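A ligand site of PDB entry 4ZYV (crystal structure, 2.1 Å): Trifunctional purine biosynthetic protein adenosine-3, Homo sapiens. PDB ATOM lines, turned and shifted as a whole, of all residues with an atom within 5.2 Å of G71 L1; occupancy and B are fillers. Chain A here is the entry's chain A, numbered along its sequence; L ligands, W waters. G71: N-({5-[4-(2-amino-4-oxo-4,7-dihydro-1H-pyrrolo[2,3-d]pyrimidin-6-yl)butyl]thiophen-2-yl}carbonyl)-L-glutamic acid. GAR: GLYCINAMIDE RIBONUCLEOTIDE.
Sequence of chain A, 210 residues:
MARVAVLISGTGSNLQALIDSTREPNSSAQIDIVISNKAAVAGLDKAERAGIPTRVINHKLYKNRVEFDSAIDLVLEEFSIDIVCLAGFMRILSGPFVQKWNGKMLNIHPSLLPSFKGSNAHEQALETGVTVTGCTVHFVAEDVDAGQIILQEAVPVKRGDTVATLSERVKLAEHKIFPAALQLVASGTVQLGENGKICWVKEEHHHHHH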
ATOM      1  N   ASN A  37      34.861 -10.960  -1.742  1.00  0.00           N
ATOM      2  CA  ASN A  37      34.187 -11.443  -2.947  1.00  0.00           C
ATOM      3  C   ASN A  37      34.262 -10.412  -4.093  1.00  0.00           C
ATOM      4  O   ASN A  37      33.884 -10.699  -5.234  1.00  0.00           O
ATOM      5  CB  ASN A  37      32.716 -11.796  -2.648  1.00  0.00           C
ATOM      6  CG  ASN A  37      31.894 -10.590  -2.235  1.00  0.00           C
ATOM      7  OD1 ASN A  37      32.296  -9.783  -1.386  1.00  0.00           O
ATOM      8  ND2 ASN A  37      30.717 -10.458  -2.849  1.00  0.00           N
ATOM      9  N   LYS A  38      34.756  -9.217  -3.763  1.00  0.00           N
ATOM     10  CA  LYS A  38      34.931  -8.142  -4.742  1.00  0.00           C
ATOM     11  C   LYS A  38      36.410  -7.762  -4.838  1.00  0.00           C
ATOM     12  O   LYS A  38      37.116  -7.636  -3.826  1.00  0.00           O
ATOM     13  CB  LYS A  38      34.106  -6.905  -4.356  1.00  0.00           C
ATOM     14  CG  LYS A  38      32.615  -7.147  -4.180  1.00  0.00           C
ATOM     15  CD  LYS A  38      31.950  -7.542  -5.497  1.00  0.00           C
ATOM     16  CE  LYS A  38      30.425  -7.571  -5.358  1.00  0.00           C
ATOM     17  NZ  LYS A  38      29.734  -7.806  -6.669  1.00  0.00           N
ATOM     18  N   ARG A  65      25.851 -21.251  -5.440  1.00  0.00           N
ATOM     19  CA  ARG A  65      26.241 -20.681  -4.161  1.00  0.00           C
ATOM     20  C   ARG A  65      27.063 -21.661  -3.294  1.00  0.00           C
ATOM     21  O   ARG A  65      27.966 -21.245  -2.571  1.00  0.00           O
ATOM     22  CB  ARG A  65      24.982 -20.220  -3.396  1.00  0.00           C
ATOM     23  CG  ARG A  65      25.269 -19.429  -2.130  1.00  0.00           C
ATOM     24  CD  ARG A  65      23.986 -18.870  -1.505  1.00  0.00           C
ATOM     25  NE  ARG A  65      23.213 -18.052  -2.431  1.00  0.00           N
ATOM     26  CZ  ARG A  65      23.323 -16.729  -2.549  1.00  0.00           C
ATOM     27  NH1 ARG A  65      24.186 -16.057  -1.798  1.00  0.00           N
ATOM     28  NH2 ARG A  65      22.561 -16.069  -3.418  1.00  0.00           N
ATOM     29  N   LEU A  86      31.980 -11.812   9.488  1.00  0.00           N
ATOM     30  CA  LEU A  86      31.453 -11.160   8.295  1.00  0.00           C
ATOM     31  C   LEU A  86      31.420  -9.640   8.518  1.00  0.00           C
ATOM     32  O   LEU A  86      30.637  -9.140   9.325  1.00  0.00           O
ATOM     33  CB  LEU A  86      30.045 -11.673   7.956  1.00  0.00           C
ATOM     34  CG  LEU A  86      29.908 -13.191   7.796  1.00  0.00           C
ATOM     35  CD1 LEU A  86      28.582 -13.546   7.155  1.00  0.00           C
ATOM     36  CD2 LEU A  86      31.059 -13.712   6.973  1.00  0.00           C
ATOM     37  N   PHE A  89      30.452  -8.077   4.533  1.00  0.00           N
ATOM     38  CA  PHE A  89      30.345  -9.138   3.541  1.00  0.00           C
ATOM     39  C   PHE A  89      28.895  -9.222   3.063  1.00  0.00           C
ATOM     40  O   PHE A  89      28.000  -9.603   3.815  1.00  0.00           O
ATOM     41  CB  PHE A  89      30.791 -10.477   4.119  1.00  0.00           C
ATOM     42  CG  PHE A  89      30.912 -11.583   3.084  1.00  0.00           C
ATOM     43  CD1 PHE A  89      31.949 -11.580   2.170  1.00  0.00           C
ATOM     44  CD2 PHE A  89      30.007 -12.627   3.076  1.00  0.00           C
ATOM     45  CE1 PHE A  89      32.059 -12.600   1.231  1.00  0.00           C
ATOM     46  CE2 PHE A  89      30.112 -13.653   2.149  1.00  0.00           C
ATOM     47  CZ  PHE A  89      31.146 -13.641   1.229  1.00  0.00           C
ATOM     48  N   MET A  90      28.667  -8.857   1.806  1.00  0.00           N
ATOM     49  CA  MET A  90      27.292  -8.697   1.325  1.00  0.00           C
ATOM     50  C   MET A  90      26.878  -9.863   0.445  1.00  0.00           C
ATOM     51  O   MET A  90      26.448  -9.679  -0.694  1.00  0.00           O
ATOM     52  CB  MET A  90      27.143  -7.371   0.571  1.00  0.00           C
ATOM     53  CG  MET A  90      27.430  -6.130   1.434  1.00  0.00           C
ATOM     54  SD  MET A  90      26.349  -5.988   2.881  1.00  0.00           S
ATOM     55  CE  MET A  90      24.804  -5.523   2.081  1.00  0.00           C
ATOM     56  N   ARG A  91      27.005 -11.075   0.989  1.00  0.00           N
ATOM     57  CA  ARG A  91      26.476 -12.265   0.331  1.00  0.00           C
ATOM     58  C   ARG A  91      25.769 -13.164   1.335  1.00  0.00           C
ATOM     59  O   ARG A  91      26.162 -13.245   2.496  1.00  0.00           O
ATOM     60  CB  ARG A  91      27.585 -13.057  -0.356  1.00  0.00           C
ATOM     61  CG  ARG A  91      28.042 -12.468  -1.650  1.00  0.00           C
ATOM     62  CD  ARG A  91      29.047 -13.382  -2.305  1.00  0.00           C
ATOM     63  NE  ARG A  91      28.484 -14.710  -2.506  1.00  0.00           N
ATOM     64  CZ  ARG A  91      27.961 -15.130  -3.649  1.00  0.00           C
ATOM     65  NH1 ARG A  91      27.944 -14.326  -4.703  1.00  0.00           N
ATOM     66  NH2 ARG A  91      27.459 -16.360  -3.731  1.00  0.00           N
ATOM     67  N   ILE A  92      24.716 -13.830   0.884  1.00  0.00           N
ATOM     68  CA  ILE A  92      24.045 -14.861   1.657  1.00  0.00           C
ATOM     69  C   ILE A  92      24.846 -16.152   1.569  1.00  0.00           C
ATOM     70  O   ILE A  92      25.224 -16.569   0.481  1.00  0.00           O
ATOM     71  CB  ILE A  92      22.622 -15.109   1.126  1.00  0.00           C
ATOM     72  CG1 ILE A  92      21.780 -13.848   1.317  1.00  0.00           C
ATOM     73  CG2 ILE A  92      21.983 -16.297   1.817  1.00  0.00           C
ATOM     74  CD1 ILE A  92      20.359 -14.004   0.830  1.00  0.00           C
ATOM     75  N   LEU A  93      25.114 -16.778   2.718  1.00  0.00           N
ATOM     76  CA  LEU A  93      25.835 -18.047   2.737  1.00  0.00           C
ATOM     77  C   LEU A  93      24.865 -19.242   2.719  1.00  0.00           C
ATOM     78  O   LEU A  93      23.799 -19.184   3.313  1.00  0.00           O
ATOM     79  CB  LEU A  93      26.733 -18.134   3.972  1.00  0.00           C
ATOM     80  CG  LEU A  93      27.733 -16.986   4.075  1.00  0.00           C
ATOM     81  CD1 LEU A  93      28.152 -16.799   5.511  1.00  0.00           C
ATOM     82  CD2 LEU A  93      28.937 -17.292   3.196  1.00  0.00           C
ATOM     83  N   SER A  94      25.267 -20.311   2.055  1.00  0.00           N
ATOM     84  CA  SER A  94      24.428 -21.505   1.959  1.00  0.00           C
ATOM     85  C   SER A  94      24.307 -22.277   3.272  1.00  0.00           C
ATOM     86  O   SER A  94      25.143 -22.149   4.170  1.00  0.00           O
ATOM     87  CB  SER A  94      24.978 -22.442   0.886  1.00  0.00           C
ATOM     88  OG  SER A  94      26.253 -22.960   1.251  1.00  0.00           O
ATOM     89  N   VAL A  98      26.896 -22.652   6.577  1.00  0.00           N
ATOM     90  CA  VAL A  98      26.454 -22.066   7.836  1.00  0.00           C
ATOM     91  C   VAL A  98      26.438 -23.124   8.933  1.00  0.00           C
ATOM     92  O   VAL A  98      26.891 -22.891  10.053  1.00  0.00           O
ATOM     93  CB  VAL A  98      25.051 -21.431   7.703  1.00  0.00           C
ATOM     94  CG1 VAL A  98      24.492 -21.040   9.079  1.00  0.00           C
ATOM     95  CG2 VAL A  98      25.105 -20.221   6.796  1.00  0.00           C
ATOM     96  N   ASN A 107      28.378 -11.967  12.446  1.00  0.00           N
ATOM     97  CA  ASN A 107      28.033 -10.958  11.459  1.00  0.00           C
ATOM     98  C   ASN A 107      27.715  -9.649  12.166  1.00  0.00           C
ATOM     99  O   ASN A 107      27.129  -9.670  13.237  1.00  0.00           O
ATOM    100  CB  ASN A 107      26.850 -11.428  10.620  1.00  0.00           C
ATOM    101  CG  ASN A 107      26.402 -10.393   9.607  1.00  0.00           C
ATOM    102  OD1 ASN A 107      27.187  -9.969   8.750  1.00  0.00           O
ATOM    103  ND2 ASN A 107      25.138  -9.995   9.670  1.00  0.00           N
ATOM    104  N   GLY A 118      18.104  -7.409   6.327  1.00  0.00           N
ATOM    105  CA  GLY A 118      18.360  -7.335   4.896  1.00  0.00           C
ATOM    106  C   GLY A 118      19.497  -6.392   4.519  1.00  0.00           C
ATOM    107  O   GLY A 118      20.255  -5.931   5.375  1.00  0.00           O
ATOM    108  N   SER A 119      19.607  -6.098   3.222  1.00  0.00           N
ATOM    109  CA  SER A 119      20.772  -5.374   2.691  1.00  0.00           C
ATOM    110  C   SER A 119      20.703  -3.841   2.764  1.00  0.00           C
ATOM    111  O   SER A 119      21.718  -3.172   2.535  1.00  0.00           O
ATOM    112  CB  SER A 119      20.975  -5.766   1.237  1.00  0.00           C
ATOM    113  OG  SER A 119      19.826  -5.360   0.500  1.00  0.00           O
ATOM    114  N   HIS A 138      25.675 -10.755  15.731  1.00  0.00           N
ATOM    115  CA  HIS A 138      24.977 -12.008  15.982  1.00  0.00           C
ATOM    116  C   HIS A 138      25.716 -13.188  15.386  1.00  0.00           C
ATOM    117  O   HIS A 138      26.463 -13.035  14.421  1.00  0.00           O
ATOM    118  CB  HIS A 138      23.547 -11.942  15.423  1.00  0.00           C
ATOM    119  CG  HIS A 138      23.492 -11.769  13.928  1.00  0.00           C
ATOM    120  ND1 HIS A 138      23.357 -12.828  13.064  1.00  0.00           N
ATOM    121  CD2 HIS A 138      23.562 -10.655  13.167  1.00  0.00           C
ATOM    122  CE1 HIS A 138      23.333 -12.380  11.816  1.00  0.00           C
ATOM    123  NE2 HIS A 138      23.455 -11.065  11.847  1.00  0.00           N
ATOM    124  N   VAL A 140      25.768 -16.260  12.958  1.00  0.00           N
ATOM    125  CA  VAL A 140      25.112 -16.512  11.681  1.00  0.00           C
ATOM    126  C   VAL A 140      24.368 -17.843  11.727  1.00  0.00           C
ATOM    127  O   VAL A 140      24.970 -18.903  11.983  1.00  0.00           O
ATOM    128  CB  VAL A 140      26.126 -16.517  10.524  1.00  0.00           C
ATOM    129  CG1 VAL A 140      25.441 -16.870   9.202  1.00  0.00           C
ATOM    130  CG2 VAL A 140      26.835 -15.169  10.427  1.00  0.00           C
ATOM    131  N   ALA A 141      23.062 -17.781  11.512  1.00  0.00           N
ATOM    132  CA  ALA A 141      22.235 -18.967  11.329  1.00  0.00           C
ATOM    133  C   ALA A 141      21.797 -19.018   9.864  1.00  0.00           C
ATOM    134  O   ALA A 141      22.080 -18.100   9.101  1.00  0.00           O
ATOM    135  CB  ALA A 141      21.039 -18.956  12.265  1.00  0.00           C
ATOM    136  N   GLU A 142      21.122 -20.080   9.462  1.00  0.00           N
ATOM    137  CA  GLU A 142      20.767 -20.233   8.066  1.00  0.00           C
ATOM    138  C   GLU A 142      19.831 -19.102   7.624  1.00  0.00           C
ATOM    139  O   GLU A 142      20.036 -18.498   6.580  1.00  0.00           O
ATOM    140  CB  GLU A 142      20.134 -21.601   7.802  1.00  0.00           C
ATOM    141  CG  GLU A 142      19.933 -21.875   6.340  1.00  0.00           C
ATOM    142  CD  GLU A 142      19.558 -23.318   6.049  1.00  0.00           C
ATOM    143  OE1 GLU A 142      19.582 -24.148   6.987  1.00  0.00           O
ATOM    144  OE2 GLU A 142      19.235 -23.616   4.883  1.00  0.00           O
ATOM    145  N   ASP A 143      18.800 -18.834   8.422  1.00  0.00           N
ATOM    146  CA  ASP A 143      17.917 -17.700   8.147  1.00  0.00           C
ATOM    147  C   ASP A 143      18.652 -16.377   8.389  1.00  0.00           C
ATOM    148  O   ASP A 143      19.208 -16.145   9.460  1.00  0.00           O
ATOM    149  CB  ASP A 143      16.649 -17.770   8.995  1.00  0.00           C
ATOM    150  CG  ASP A 143      15.636 -18.769   8.454  1.00  0.00           C
ATOM    151  OD1 ASP A 143      15.617 -18.978   7.226  1.00  0.00           O
ATOM    152  OD2 ASP A 143      14.870 -19.335   9.259  1.00  0.00           O
ATOM    153  N   VAL A 144      18.643 -15.526   7.365  1.00  0.00           N
ATOM    154  CA  VAL A 144      19.430 -14.287   7.366  1.00  0.00           C
ATOM    155  C   VAL A 144      19.044 -13.325   8.494  1.00  0.00           C
ATOM    156  O   VAL A 144      17.864 -13.053   8.718  1.00  0.00           O
ATOM    157  CB  VAL A 144      19.312 -13.581   5.992  1.00  0.00           C
ATOM    158  CG1 VAL A 144      20.096 -12.283   5.990  1.00  0.00           C
ATOM    159  CG2 VAL A 144      19.824 -14.494   4.898  1.00  0.00           C
ATOM    160  N   ASP A 145      20.062 -12.827   9.212  1.00  0.00           N
ATOM    161  CA  ASP A 145      19.885 -11.899  10.322  1.00  0.00           C
ATOM    162  C   ASP A 145      18.922 -12.413  11.405  1.00  0.00           C
ATOM    163  O   ASP A 145      18.225 -11.615  12.043  1.00  0.00           O
ATOM    164  CB  ASP A 145      19.388 -10.535   9.803  1.00  0.00           C
ATOM    165  CG  ASP A 145      20.317  -9.934   8.753  1.00  0.00           C
ATOM    166  OD1 ASP A 145      21.538 -10.239   8.776  1.00  0.00           O
ATOM    167  OD2 ASP A 145      19.818  -9.170   7.899  1.00  0.00           O
ATOM    168  N   ALA A 146      18.876 -13.724  11.603  1.00  0.00           N
ATOM    169  CA  ALA A 146      17.979 -14.337  12.583  1.00  0.00           C
ATOM    170  C   ALA A 146      18.751 -15.095  13.674  1.00  0.00           C
ATOM    171  O   ALA A 146      18.166 -15.592  14.627  1.00  0.00           O
ATOM    172  CB  ALA A 146      16.968 -15.274  11.894  1.00  0.00           C
HETATM  173  N1  G71 L   1      23.961 -15.588   5.294  1.00  0.00           N
HETATM  174  C2  G71 L   1      23.238 -16.396   6.072  1.00  0.00           C
HETATM  175  N3  G71 L   1      22.791 -15.967   7.267  1.00  0.00           N
HETATM  176  C4  G71 L   1      23.052 -14.728   7.731  1.00  0.00           C
HETATM  177  N5  G71 L   1      24.956 -13.382   5.086  1.00  0.00           N
HETATM  178  C6  G71 L   1      25.013 -12.287   5.856  1.00  0.00           C
HETATM  179  C7  G71 L   1      24.294 -12.549   7.036  1.00  0.00           C
HETATM  180  C8  G71 L   1      23.825 -13.867   6.937  1.00  0.00           C
HETATM  181  C9  G71 L   1      24.261 -14.335   5.689  1.00  0.00           C
HETATM  182  O10 G71 L   1      22.558 -14.362   8.965  1.00  0.00           O
HETATM  183  N11 G71 L   1      22.926 -17.710   5.629  1.00  0.00           N
HETATM  184  S12 G71 L   1      23.468  -9.517   1.175  1.00  0.00           S
HETATM  185  C13 G71 L   1      22.314 -10.094   0.105  1.00  0.00           C
HETATM  186  C14 G71 L   1      21.123 -10.180   0.858  1.00  0.00           C
HETATM  187  C15 G71 L   1      21.225  -9.777   2.224  1.00  0.00           C
HETATM  188  C16 G71 L   1      22.530  -9.363   2.556  1.00  0.00           C
HETATM  189  C17 G71 L   1      22.537 -10.477  -1.326  1.00  0.00           C
HETATM  190  O18 G71 L   1      21.599 -10.895  -1.979  1.00  0.00           O
HETATM  191  N19 G71 L   1      23.844 -10.375  -1.902  1.00  0.00           N
HETATM  192  C20 G71 L   1      24.114 -10.764  -3.253  1.00  0.00           C
HETATM  193  C21 G71 L   1      25.425 -10.180  -3.689  1.00  0.00           C
HETATM  194  C22 G71 L   1      25.287  -9.428  -4.968  1.00  0.00           C
HETATM  195  C23 G71 L   1      26.251  -8.287  -5.027  1.00  0.00           C
HETATM  196  O24 G71 L   1      27.308  -8.369  -5.708  1.00  0.00           O
HETATM  197  O25 G71 L   1      25.998  -7.223  -4.401  1.00  0.00           O
HETATM  198  C26 G71 L   1      24.201 -12.258  -3.314  1.00  0.00           C
HETATM  199  O27 G71 L   1      24.298 -12.848  -4.420  1.00  0.00           O
HETATM  200  O28 G71 L   1      24.164 -12.954  -2.259  1.00  0.00           O
HETATM  201  C29 G71 L   1      25.683 -11.015   5.497  1.00  0.00           C
HETATM  202  C30 G71 L   1      24.964 -10.313   4.374  1.00  0.00           C
HETATM  203  C31 G71 L   1      23.527 -10.042   4.696  1.00  0.00           C
HETATM  204  C32 G71 L   1      22.987  -8.891   3.899  1.00  0.00           C
HETATM  205  C1  GAR L   2      28.644  -1.883   7.767  1.00  0.00           C
HETATM  206  O6  GAR L   2      27.863  -0.743   8.120  1.00  0.00           O
HETATM  207  C2  GAR L   2      27.859  -3.141   8.089  1.00  0.00           C
HETATM  208  O8  GAR L   2      27.062  -3.043   9.285  1.00  0.00           O
HETATM  209  C3  GAR L   2      26.994  -3.308   6.849  1.00  0.00           C
HETATM  210  O4  GAR L   2      27.833  -2.875   5.777  1.00  0.00           O
HETATM  211  C5  GAR L   2      28.779  -1.901   6.255  1.00  0.00           C
HETATM  212  C10 GAR L   2      30.195  -2.280   5.836  1.00  0.00           C
HETATM  213  O12 GAR L   2      31.115  -1.228   6.128  1.00  0.00           O
HETATM  214  N19 GAR L   2      26.577  -4.680   6.684  1.00  0.00           N
HETATM  215  C21 GAR L   2      25.365  -4.989   6.244  1.00  0.00           C
HETATM  216  O22 GAR L   2      24.542  -4.156   5.863  1.00  0.00           O
HETATM  217  C23 GAR L   2      25.100  -6.489   6.243  1.00  0.00           C
HETATM  218  N24 GAR L   2      23.681  -6.807   6.218  1.00  0.00           N
HETATM  219  P15 GAR L   2      32.715  -1.513   6.153  1.00  0.00           P
HETATM  220  O16 GAR L   2      32.890  -2.417   7.356  1.00  0.00           O
HETATM  221  O17 GAR L   2      33.324  -0.120   6.263  1.00  0.00           O
HETATM  222  O18 GAR L   2      33.057  -2.189   4.824  1.00  0.00           O
HETATM  223  O   HOH W   1      28.451  -6.023  -2.447  1.00  0.00           O
HETATM  224  O   HOH W   2      28.512  -8.533  -2.414  1.00  0.00           O
HETATM  225  O   HOH W   3      21.431 -15.448  10.920  1.00  0.00           O
HETATM  226  O   HOH W   4      28.402  -9.090   6.484  1.00  0.00           O
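O of Arg 91 lies within hydrogen-bond range of N5 of G71 L1 (2.9 Å).
O of Leu 93 is in hydrogen-bond range of N11 of G71 L1 (2.9 Å).
The backbone carbonyl oxygen (O) of Met 90 lies within hydrogen-bond range of a nitrogen (N19) of G71 L1 (3.0 Å).
N11 of G71 L1 sits at hydrogen-bond distance from O of Glu 142 (3.1 Å).
NH1 of Arg 91 lies within salt-bridge range of O27 of G71 L1 (3.9 Å).
O28 of G71 L1 is in salt-bridge range of NH1 of Arg 65 (3.1 Å).
The side-chain amino group of Lys 38 is in salt-bridge range of an oxygen (O24) of G71 L1.
The backbone NH (N) of Asp 145 lies within hydrogen-bond range of an oxygen (O10) of G71 L1, 2.9 Å away.
A nitrogen (N1) of G71 L1 is in hydrogen-bond range of the backbone NH (N) of Leu 93, at 3.1 Å.
The backbone NH (N) of Ile 92 sits at hydrogen-bond distance from an oxygen (O28) of G71 L1.
The guanidinium group (NH1) of Arg 65 sits at hydrogen-bond distance from the backbone carbonyl oxygen (O) of Ile 92.
The side-chain carboxylate (OD2) of Asp 145 sits at hydrogen-bond distance from the backbone NH (N) of Gly 118 (2.9 Å).
O of His 138 lies within hydrogen-bond range of N of Asn 107 (3.0 Å).
Water W2 lies within hydrogen-bond range of O of Met 90 (2.9 Å), ND2 of Asn 37 (3.0 Å) and O25 of G71 L1 (3.5 Å).
Water W4 lies within hydrogen-bond range of the side-chain amide oxygen of Asn 107 (2.7 Å) and the backbone carbonyl oxygen of Phe 89 (2.7 Å).
A nitrogen (N3) of G71 L1 sits close to the backbone carbonyl oxygen (O) of Ala 141 (2.9 Å).
O of Phe 89 touches C30 of G71 L1, 3.2 Å away.
Val 98 touches G71 L1 (CG2 to N11, 3.5 Å).
OD1 of Asn 107 touches C29 of G71 L1, 3.7 Å away.
CE1 of His 138 touches O10 of G71 L1 (3.6 Å).
Val 140 touches G71 L1.
O of Asp 143 touches O10 of G71 L1, at 3.8 Å.
Val 144 touches G71 L1.
Hydrophobic or aromatic side chains that line G71 L1: Ile 92, Leu 93, Val 98, His 138 and Val 140.
16 residues have an atom within 4 Å of G71 L1: Lys 38, Arg 65, Phe 89, Met 90, Arg 91, Ile 92, Leu 93, Val 98, Asn 107, His 138, Val 140, Ala 141, Glu 142, Asp 143, Val 144 and Asp 145.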
